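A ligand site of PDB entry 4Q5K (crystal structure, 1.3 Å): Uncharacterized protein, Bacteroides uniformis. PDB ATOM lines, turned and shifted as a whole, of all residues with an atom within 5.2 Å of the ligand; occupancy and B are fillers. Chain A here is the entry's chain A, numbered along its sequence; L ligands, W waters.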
ATOM      1  N   TYR A  19      24.932   9.049  28.565  1.00  0.00           N
ATOM      2  CA  TYR A  19      24.384   8.715  27.265  1.00  0.00           C
ATOM      3  C   TYR A  19      25.490   8.845  26.214  1.00  0.00           C
ATOM      4  O   TYR A  19      26.114   9.898  26.111  1.00  0.00           O
ATOM      5  CB  TYR A  19      23.239   9.684  26.910  1.00  0.00           C
ATOM      6  CG  TYR A  19      22.533   9.303  25.619  1.00  0.00           C
ATOM      7  CD1 TYR A  19      23.119   9.576  24.387  1.00  0.00           C
ATOM      8  CD2 TYR A  19      21.309   8.650  25.633  1.00  0.00           C
ATOM      9  CE1 TYR A  19      22.506   9.228  23.206  1.00  0.00           C
ATOM     10  CE2 TYR A  19      20.686   8.290  24.436  1.00  0.00           C
ATOM     11  CZ  TYR A  19      21.301   8.582  23.234  1.00  0.00           C
ATOM     12  OH  TYR A  19      20.731   8.242  22.032  1.00  0.00           O
ATOM     13  N   HIS A  22      25.825   4.943  19.567  1.00  0.00           N
ATOM     14  CA  HIS A  22      26.622   4.051  18.715  1.00  0.00           C
ATOM     15  C   HIS A  22      27.603   3.178  19.501  1.00  0.00           C
ATOM     16  O   HIS A  22      28.585   2.702  18.924  1.00  0.00           O
ATOM     17  CB  HIS A  22      27.336   4.850  17.614  1.00  0.00           C
ATOM     18  CG  HIS A  22      26.422   5.697  16.823  1.00  0.00           C
ATOM     19  ND1 HIS A  22      25.275   5.225  16.233  1.00  0.00           N
ATOM     20  CD2 HIS A  22      26.486   7.020  16.502  1.00  0.00           C
ATOM     21  CE1 HIS A  22      24.672   6.206  15.588  1.00  0.00           C
ATOM     22  NE2 HIS A  22      25.372   7.310  15.749  1.00  0.00           N
ATOM     23  N   LEU A  24      27.515   0.124  20.248  1.00  0.00           N
ATOM     24  CA  LEU A  24      27.617  -1.236  19.713  1.00  0.00           C
ATOM     25  C   LEU A  24      28.301  -1.305  18.359  1.00  0.00           C
ATOM     26  O   LEU A  24      28.456  -2.409  17.820  1.00  0.00           O
ATOM     27  CB  LEU A  24      26.243  -1.852  19.621  1.00  0.00           C
ATOM     28  CG  LEU A  24      25.378  -1.798  20.889  1.00  0.00           C
ATOM     29  CD1 LEU A  24      24.153  -2.632  20.719  1.00  0.00           C
ATOM     30  CD2 LEU A  24      26.146  -2.246  22.108  1.00  0.00           C
ATOM     31  N   GLU A  25      28.761  -0.177  17.825  1.00  0.00           N
ATOM     32  CA  GLU A  25      29.153  -0.109  16.418  1.00  0.00           C
ATOM     33  C   GLU A  25      30.645  -0.122  16.131  1.00  0.00           C
ATOM     34  O   GLU A  25      31.091   0.501  15.149  1.00  0.00           O
ATOM     35  CB  GLU A  25      28.544   1.114  15.744  1.00  0.00           C
ATOM     36  CG  GLU A  25      27.097   1.378  16.048  1.00  0.00           C
ATOM     37  CD  GLU A  25      26.138   0.210  15.850  1.00  0.00           C
ATOM     38  OE1 GLU A  25      26.511  -0.819  15.267  1.00  0.00           O
ATOM     39  OE2 GLU A  25      24.972   0.328  16.302  1.00  0.00           O
ATOM     40  N   ASP A  40      22.662   3.949  25.482  1.00  0.00           N
ATOM     41  CA  ASP A  40      21.559   4.665  24.851  1.00  0.00           C
ATOM     42  C   ASP A  40      20.249   4.083  25.335  1.00  0.00           C
ATOM     43  O   ASP A  40      20.240   3.198  26.203  1.00  0.00           O
ATOM     44  CB  ASP A  40      21.710   4.731  23.324  1.00  0.00           C
ATOM     45  CG  ASP A  40      21.610   3.397  22.635  1.00  0.00           C
ATOM     46  OD1 ASP A  40      20.822   2.537  23.093  1.00  0.00           O
ATOM     47  OD2 ASP A  40      22.304   3.228  21.610  1.00  0.00           O
ATOM     48  N   CYS A  41      19.117   4.557  24.813  1.00  0.00           N
ATOM     49  CA  CYS A  41      17.844   4.148  25.421  1.00  0.00           C
ATOM     50  C   CYS A  41      17.606   2.651  25.294  1.00  0.00           C
ATOM     51  O   CYS A  41      16.988   2.042  26.170  1.00  0.00           O
ATOM     52  CB  CYS A  41      16.663   4.918  24.830  1.00  0.00           C
ATOM     53  SG  CYS A  41      16.366   4.594  23.101  1.00  0.00           S
ATOM     54  N   THR A  42      18.101   2.058  24.202  1.00  0.00           N
ATOM     55  CA  THR A  42      17.915   0.644  23.956  1.00  0.00           C
ATOM     56  C   THR A  42      18.918  -0.200  24.732  1.00  0.00           C
ATOM     57  O   THR A  42      18.531  -1.172  25.380  1.00  0.00           O
ATOM     58  CB  THR A  42      17.955   0.344  22.451  1.00  0.00           C
ATOM     59  OG1 THR A  42      16.918   1.088  21.807  1.00  0.00           O
ATOM     60  CG2 THR A  42      17.809  -1.123  22.156  1.00  0.00           C
ATOM     61  N   THR A  43      20.185   0.151  24.694  1.00  0.00           N
ATOM     62  CA  THR A  43      21.136  -0.675  25.415  1.00  0.00           C
ATOM     63  C   THR A  43      20.882  -0.632  26.921  1.00  0.00           C
ATOM     64  O   THR A  43      21.047  -1.639  27.599  1.00  0.00           O
ATOM     65  CB  THR A  43      22.626  -0.356  25.084  1.00  0.00           C
ATOM     66  OG1 THR A  43      23.000   0.910  25.637  1.00  0.00           O
ATOM     67  CG2 THR A  43      22.913  -0.387  23.593  1.00  0.00           C
ATOM     68  N   TYR A  84      26.038  -8.251  11.363  1.00  0.00           N
ATOM     69  CA  TYR A  84      25.309  -7.070  11.805  1.00  0.00           C
ATOM     70  C   TYR A  84      23.791  -7.273  11.793  1.00  0.00           C
ATOM     71  O   TYR A  84      23.102  -6.803  12.694  1.00  0.00           O
ATOM     72  CB  TYR A  84      25.679  -5.913  10.901  1.00  0.00           C
ATOM     73  CG  TYR A  84      24.969  -4.619  11.173  1.00  0.00           C
ATOM     74  CD1 TYR A  84      25.246  -3.881  12.324  1.00  0.00           C
ATOM     75  CD2 TYR A  84      24.046  -4.106  10.271  1.00  0.00           C
ATOM     76  CE1 TYR A  84      24.626  -2.666  12.566  1.00  0.00           C
ATOM     77  CE2 TYR A  84      23.405  -2.923  10.531  1.00  0.00           C
ATOM     78  CZ  TYR A  84      23.680  -2.196  11.655  1.00  0.00           C
ATOM     79  OH  TYR A  84      23.044  -1.013  11.849  1.00  0.00           O
ATOM     80  N   ARG A  87      21.533  -8.728  14.752  1.00  0.00           N
ATOM     81  CA  ARG A  87      21.130  -7.900  15.894  1.00  0.00           C
ATOM     82  C   ARG A  87      19.679  -7.451  15.666  1.00  0.00           C
ATOM     83  O   ARG A  87      19.309  -7.130  14.531  1.00  0.00           O
ATOM     84  CB  ARG A  87      22.050  -6.657  16.030  1.00  0.00           C
ATOM     85  CG  ARG A  87      22.106  -6.086  17.414  1.00  0.00           C
ATOM     86  CD  ARG A  87      22.660  -4.725  17.471  1.00  0.00           C
ATOM     87  NE  ARG A  87      24.007  -4.644  16.914  1.00  0.00           N
ATOM     88  CZ  ARG A  87      24.598  -3.504  16.544  1.00  0.00           C
ATOM     89  NH1 ARG A  87      23.971  -2.336  16.675  1.00  0.00           N
ATOM     90  NH2 ARG A  87      25.811  -3.508  16.021  1.00  0.00           N
ATOM     91  N   HIS A  89      17.641  -4.949  15.462  1.00  0.00           N
ATOM     92  CA  HIS A  89      17.663  -3.497  15.303  1.00  0.00           C
ATOM     93  C   HIS A  89      16.319  -2.832  15.491  1.00  0.00           C
ATOM     94  O   HIS A  89      16.230  -1.763  16.077  1.00  0.00           O
ATOM     95  CB  HIS A  89      18.214  -3.135  13.916  1.00  0.00           C
ATOM     96  CG  HIS A  89      19.615  -3.576  13.709  1.00  0.00           C
ATOM     97  ND1 HIS A  89      20.662  -3.014  14.402  1.00  0.00           N
ATOM     98  CD2 HIS A  89      20.150  -4.522  12.913  1.00  0.00           C
ATOM     99  CE1 HIS A  89      21.786  -3.611  14.048  1.00  0.00           C
ATOM    100  NE2 HIS A  89      21.508  -4.513  13.130  1.00  0.00           N
ATOM    101  N   TYR A  90      15.283  -3.441  14.919  1.00  0.00           N
ATOM    102  CA  TYR A  90      13.942  -2.873  15.039  1.00  0.00           C
ATOM    103  C   TYR A  90      13.245  -3.386  16.286  1.00  0.00           C
ATOM    104  O   TYR A  90      13.216  -4.582  16.554  1.00  0.00           O
ATOM    105  CB  TYR A  90      13.129  -3.209  13.819  1.00  0.00           C
ATOM    106  CG  TYR A  90      13.547  -2.471  12.583  1.00  0.00           C
ATOM    107  CD1 TYR A  90      13.338  -1.097  12.466  1.00  0.00           C
ATOM    108  CD2 TYR A  90      14.143  -3.140  11.527  1.00  0.00           C
ATOM    109  CE1 TYR A  90      13.685  -0.417  11.318  1.00  0.00           C
ATOM    110  CE2 TYR A  90      14.498  -2.440  10.376  1.00  0.00           C
ATOM    111  CZ  TYR A  90      14.275  -1.095  10.258  1.00  0.00           C
ATOM    112  OH  TYR A  90      14.545  -0.376   9.098  1.00  0.00           O
ATOM    113  N   ILE A  91      12.645  -2.491  17.061  1.00  0.00           N
ATOM    114  CA  ILE A  91      12.047  -2.887  18.335  1.00  0.00           C
ATOM    115  C   ILE A  91      10.863  -3.831  18.133  1.00  0.00           C
ATOM    116  O   ILE A  91      10.692  -4.749  18.928  1.00  0.00           O
ATOM    117  CB  ILE A  91      11.712  -1.651  19.190  1.00  0.00           C
ATOM    118  CG1 ILE A  91      13.003  -0.878  19.494  1.00  0.00           C
ATOM    119  CG2 ILE A  91      11.023  -2.033  20.443  1.00  0.00           C
ATOM    120  CD1 ILE A  91      14.181  -1.676  20.038  1.00  0.00           C
ATOM    121  N   TYR A 122      13.042   2.160   7.564  1.00  0.00           N
ATOM    122  CA  TYR A 122      13.930   3.300   7.842  1.00  0.00           C
ATOM    123  C   TYR A 122      15.389   3.014   7.538  1.00  0.00           C
ATOM    124  O   TYR A 122      16.058   3.847   6.908  1.00  0.00           O
ATOM    125  CB  TYR A 122      13.783   3.729   9.314  1.00  0.00           C
ATOM    126  CG  TYR A 122      14.481   5.017   9.682  1.00  0.00           C
ATOM    127  CD1 TYR A 122      13.867   6.244   9.519  1.00  0.00           C
ATOM    128  CD2 TYR A 122      15.775   4.999  10.166  1.00  0.00           C
ATOM    129  CE1 TYR A 122      14.534   7.419   9.847  1.00  0.00           C
ATOM    130  CE2 TYR A 122      16.437   6.161  10.500  1.00  0.00           C
ATOM    131  CZ  TYR A 122      15.807   7.367  10.350  1.00  0.00           C
ATOM    132  OH  TYR A 122      16.456   8.522  10.692  1.00  0.00           O
ATOM    133  N   MET A 123      15.907   1.891   7.999  1.00  0.00           N
ATOM    134  CA  MET A 123      17.338   1.627   7.884  1.00  0.00           C
ATOM    135  C   MET A 123      17.782   1.445   6.435  1.00  0.00           C
ATOM    136  O   MET A 123      18.779   2.048   6.022  1.00  0.00           O
ATOM    137  CB  MET A 123      17.742   0.417   8.698  1.00  0.00           C
ATOM    138  CG  MET A 123      17.525   0.619  10.188  1.00  0.00           C
ATOM    139  SD  MET A 123      17.932  -0.954  11.229  1.00  0.00           S
ATOM    140  CE  MET A 123      19.837  -0.892  11.142  1.00  0.00           C
ATOM    141  N   TYR A 130      23.987   4.415   9.283  1.00  0.00           N
ATOM    142  CA  TYR A 130      24.426   3.199   9.948  1.00  0.00           C
ATOM    143  C   TYR A 130      25.752   2.742   9.339  1.00  0.00           C
ATOM    144  O   TYR A 130      25.815   2.428   8.147  1.00  0.00           O
ATOM    145  CB  TYR A 130      23.364   2.097   9.798  1.00  0.00           C
ATOM    146  CG  TYR A 130      22.023   2.477  10.405  1.00  0.00           C
ATOM    147  CD1 TYR A 130      21.757   2.197  11.726  1.00  0.00           C
ATOM    148  CD2 TYR A 130      21.055   3.140   9.653  1.00  0.00           C
ATOM    149  CE1 TYR A 130      20.556   2.563  12.286  1.00  0.00           C
ATOM    150  CE2 TYR A 130      19.868   3.535  10.214  1.00  0.00           C
ATOM    151  CZ  TYR A 130      19.610   3.221  11.541  1.00  0.00           C
ATOM    152  OH  TYR A 130      18.400   3.600  12.085  1.00  0.00           O
ATOM    153  N   LEU A 186       9.478   3.840  10.456  1.00  0.00           N
ATOM    154  CA  LEU A 186       9.989   3.493  11.769  1.00  0.00           C
ATOM    155  C   LEU A 186       8.844   3.214  12.730  1.00  0.00           C
ATOM    156  O   LEU A 186       7.835   3.942  12.741  1.00  0.00           O
ATOM    157  CB  LEU A 186      10.866   4.624  12.308  1.00  0.00           C
ATOM    158  CG  LEU A 186      11.599   4.380  13.625  1.00  0.00           C
ATOM    159  CD1 LEU A 186      12.594   3.242  13.488  1.00  0.00           C
ATOM    160  CD2 LEU A 186      12.294   5.654  14.087  1.00  0.00           C
ATOM    161  N   VAL A 188       9.300   2.431  16.342  1.00  0.00           N
ATOM    162  CA  VAL A 188       9.577   2.880  17.700  1.00  0.00           C
ATOM    163  C   VAL A 188      10.718   3.862  17.646  1.00  0.00           C
ATOM    164  O   VAL A 188      11.661   3.631  16.876  1.00  0.00           O
ATOM    165  CB  VAL A 188       9.906   1.670  18.617  1.00  0.00           C
ATOM    166  CG1 VAL A 188      10.547   2.088  19.941  1.00  0.00           C
ATOM    167  CG2 VAL A 188       8.681   0.853  18.865  1.00  0.00           C
ATOM    168  N   ALA A 189      10.655   4.939  18.433  1.00  0.00           N
ATOM    169  CA  ALA A 189      11.665   5.995  18.476  1.00  0.00           C
ATOM    170  C   ALA A 189      12.452   6.114  19.772  1.00  0.00           C
ATOM    171  O   ALA A 189      13.503   6.749  19.780  1.00  0.00           O
ATOM    172  CB  ALA A 189      11.002   7.327  18.199  1.00  0.00           C
ATOM    173  N   HIS A 190      11.960   5.523  20.860  1.00  0.00           N
ATOM    174  CA  HIS A 190      12.569   5.722  22.159  1.00  0.00           C
ATOM    175  C   HIS A 190      12.018   4.629  23.081  1.00  0.00           C
ATOM    176  O   HIS A 190      10.963   4.076  22.834  1.00  0.00           O
ATOM    177  CB  HIS A 190      12.248   7.135  22.677  1.00  0.00           C
ATOM    178  CG  HIS A 190      12.995   7.513  23.920  1.00  0.00           C
ATOM    179  ND1 HIS A 190      14.302   7.160  24.124  1.00  0.00           N
ATOM    180  CD2 HIS A 190      12.614   8.194  25.025  1.00  0.00           C
ATOM    181  CE1 HIS A 190      14.719   7.634  25.287  1.00  0.00           C
ATOM    182  NE2 HIS A 190      13.702   8.262  25.849  1.00  0.00           N
ATOM    183  N   MET A 191      12.731   4.364  24.156  1.00  0.00           N
ATOM    184  CA  MET A 191      12.351   3.353  25.140  1.00  0.00           C
ATOM    185  C   MET A 191      12.767   3.766  26.529  1.00  0.00           C
ATOM    186  O   MET A 191      13.691   4.572  26.691  1.00  0.00           O
ATOM    187  CB  MET A 191      13.074   2.014  24.868  1.00  0.00           C
ATOM    188  CG  MET A 191      12.962   1.481  23.506  1.00  0.00           C
ATOM    189  SD  MET A 191      13.889  -0.119  23.265  1.00  0.00           S
ATOM    190  CE  MET A 191      12.536  -1.238  24.064  1.00  0.00           C
ATOM    191  N   SER A 208      19.129  11.495  25.522  1.00  0.00           N
ATOM    192  CA  SER A 208      20.121  12.110  24.661  1.00  0.00           C
ATOM    193  C   SER A 208      20.221  13.606  24.950  1.00  0.00           C
ATOM    194  O   SER A 208      21.297  14.190  24.811  1.00  0.00           O
ATOM    195  CB  SER A 208      19.791  11.856  23.187  1.00  0.00           C
ATOM    196  OG  SER A 208      18.577  12.496  22.825  1.00  0.00           O
HETATM  197  C1  LIG L   1      18.593   1.214  17.901  1.00  0.00           C
HETATM  198  O1  LIG L   1      17.976   2.449  17.753  1.00  0.00           O
HETATM  199  C2  LIG L   1      19.073   0.806  16.520  1.00  0.00           C
HETATM  200  C3  LIG L   1      19.950  -0.448  16.612  1.00  0.00           C
HETATM  201  O2  LIG L   1      20.623  -0.613  15.379  1.00  0.00           O
HETATM  202  C4  LIG L   1      20.994  -0.351  17.718  1.00  0.00           C
HETATM  203  O3  LIG L   1      17.970   2.603  14.616  1.00  0.00           O
HETATM  204  C5  LIG L   1      17.452   1.494  14.787  1.00  0.00           C
HETATM  205  C6  LIG L   1      16.199   1.087  14.078  1.00  0.00           C
HETATM  206  N1  LIG L   1      17.952   0.584  15.637  1.00  0.00           N
HETATM  207  O4  LIG L   1      21.569  -1.639  17.932  1.00  0.00           O
HETATM  208  C7  LIG L   1      20.343   0.111  19.011  1.00  0.00           C
HETATM  209  C8  LIG L   1      21.337   0.322  20.152  1.00  0.00           C
HETATM  210  O5  LIG L   1      22.328   1.307  19.841  1.00  0.00           O
HETATM  211  O6  LIG L   1      19.682   1.367  18.787  1.00  0.00           O
HETATM  212  C9  LIG L   1      17.136   2.909  18.824  1.00  0.00           C
HETATM  213  C10 LIG L   1      16.921   4.385  18.512  1.00  0.00           C
HETATM  214  O7  LIG L   1      16.781   5.117  19.739  1.00  0.00           O
HETATM  215  C11 LIG L   1      17.890   6.008  19.964  1.00  0.00           C
HETATM  216  C12 LIG L   1      19.056   5.218  20.535  1.00  0.00           C
HETATM  217  C13 LIG L   1      17.440   7.172  20.858  1.00  0.00           C
HETATM  218  O8  LIG L   1      18.288   7.808  21.487  1.00  0.00           O
HETATM  219  O9  LIG L   1      16.194   7.386  20.861  1.00  0.00           O
HETATM  220  C14 LIG L   1      15.828   2.122  18.891  1.00  0.00           C
HETATM  221  O10 LIG L   1      15.104   2.316  17.650  1.00  0.00           O
HETATM  222  C15 LIG L   1      14.844   2.664  19.919  1.00  0.00           C
HETATM  223  O11 LIG L   1      14.082   3.638  19.169  1.00  0.00           O
HETATM  224  C16 LIG L   1      14.585   3.608  17.833  1.00  0.00           C
HETATM  225  C17 LIG L   1      15.695   4.638  17.626  1.00  0.00           C
HETATM  226  N2  LIG L   1      16.065   4.706  16.221  1.00  0.00           N
HETATM  227  C18 LIG L   1      15.749   5.706  15.425  1.00  0.00           C
HETATM  228  O12 LIG L   1      15.118   6.677  15.840  1.00  0.00           O
HETATM  229  C19 LIG L   1      16.195   5.589  13.995  1.00  0.00           C
HETATM  230  O   HOH W   1      19.579  -3.267  18.637  1.00  0.00           O
HETATM  231  O   HOH W   2      25.010   1.189  19.040  1.00  0.00           O
HETATM  232  O   HOH W   3      20.756  -2.446  21.382  1.00  0.00           O
HETATM  233  O   HOH W   4      15.839   9.764  19.532  1.00  0.00           O
HETATM  234  O   HOH W   5      17.156   8.208  17.344  1.00  0.00           O
HETATM  235  O   HOH W   6      19.841   4.422  15.690  1.00  0.00           O
HETATM  236  O   HOH W   7      13.613   8.656  14.840  1.00  0.00           O
HETATM  237  O   HOH W   8      14.199   8.891  17.829  1.00  0.00           O
HETATM  238  O   HOH W   9      23.074   0.148  14.253  1.00  0.00           O
HETATM  239  O   HOH W  10      21.528   3.412  17.556  1.00  0.00           O
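Water W2 lies within hydrogen-bond range of O5 of the ligand (2.8 Å), OE2 of Glu 25 (2.9 Å) and N of Leu 24 (3.0 Å). Water W9 lies within hydrogen-bond range of the side-chain hydroxyl (OH) of Tyr 84 (2.7 Å), the side-chain carboxylate (OE2) of Glu 25 (2.8 Å) and an oxygen (O2) of the ligand (2.8 Å). Water W8 lies within hydrogen-bond range of O of Ala 189 and O12 of the ligand.
NE2 of His 89 lies within hydrogen-bond range of O of Tyr 84. The side-chain carboxylate (OD1) of Asp 40 is in hydrogen-bond range of the backbone NH (N) of Thr 42, 3.0 Å away. The guanidinium group (NH2) of Arg 87 is in hydrogen-bond range of the backbone carbonyl oxygen (O) of Leu 24 (3.4 Å). OE2 of Glu 25 lies within salt-bridge range of NH1 of Arg 87, at 2.9 Å. The side-chain hydroxyl of Thr 42 is in hydrogen-bond range of the side-chain sulfur of Cys 41 (3.8 Å). The side-chain sulfur (SD) of Met 191 sits at hydrogen-bond distance from the side-chain hydroxyl (OG1) of Thr 42 (3.6 Å). The side-chain sulfur (SG) of Cys 41 is in hydrogen-bond range of the backbone NH (N) of Met 191, at 3.8 Å. The backbone NH (N) of Met 123 is in hydrogen-bond range of the side-chain hydroxyl (OH) of Tyr 90 (2.9 Å).
The side-chain hydroxyl (OH) of Tyr 19 lies within hydrogen-bond range of an oxygen (O8) of the ligand (2.5 Å). The backbone carbonyl oxygen of His 89 is in hydrogen-bond range of a nitrogen (N1) of the ligand. ND1 of His 89 is in hydrogen-bond range of O2 of the ligand. The side-chain carboxylate (OD2) of Asp 40 is in hydrogen-bond range of an oxygen (O5) of the ligand, 2.6 Å away. O3 of the ligand lies within hydrogen-bond range of OH of Tyr 130 (2.8 Å). O4 of the ligand lies within hydrogen-bond range of NH1 of Arg 87. O of Ala 189 sits close to O9 of the ligand (3.0 Å). The backbone NH (N) of His 190 is in hydrogen-bond range of an oxygen (O11) of the ligand, at 3.3 Å. SG of Cys 41 sits at hydrogen-bond distance from O7 of the ligand (3.4 Å).
O11 of the ligand lies close to O of Val 188 (3.3 Å). Leu 24 touches the ligand (CD1 to O4, 3.9 Å). Thr 42 touches the ligand (OG1 to C15, 3.2 Å). CG2 of Thr 43 touches C8 of the ligand, at 3.9 Å. Tyr 90 touches the ligand. Tyr 122 touches the ligand. Met 123 touches the ligand. CD2 of Leu 186 touches O12 of the ligand (3.5 Å). 16 residues have an atom within 4 Å of the ligand: Tyr 19, Leu 24, Asp 40, Cys 41, Thr 42, Thr 43, Arg 87, His 89, Tyr 90, Tyr 122, Met 123, Tyr 130, Leu 186, Val 188, Ala 189 and His 190.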
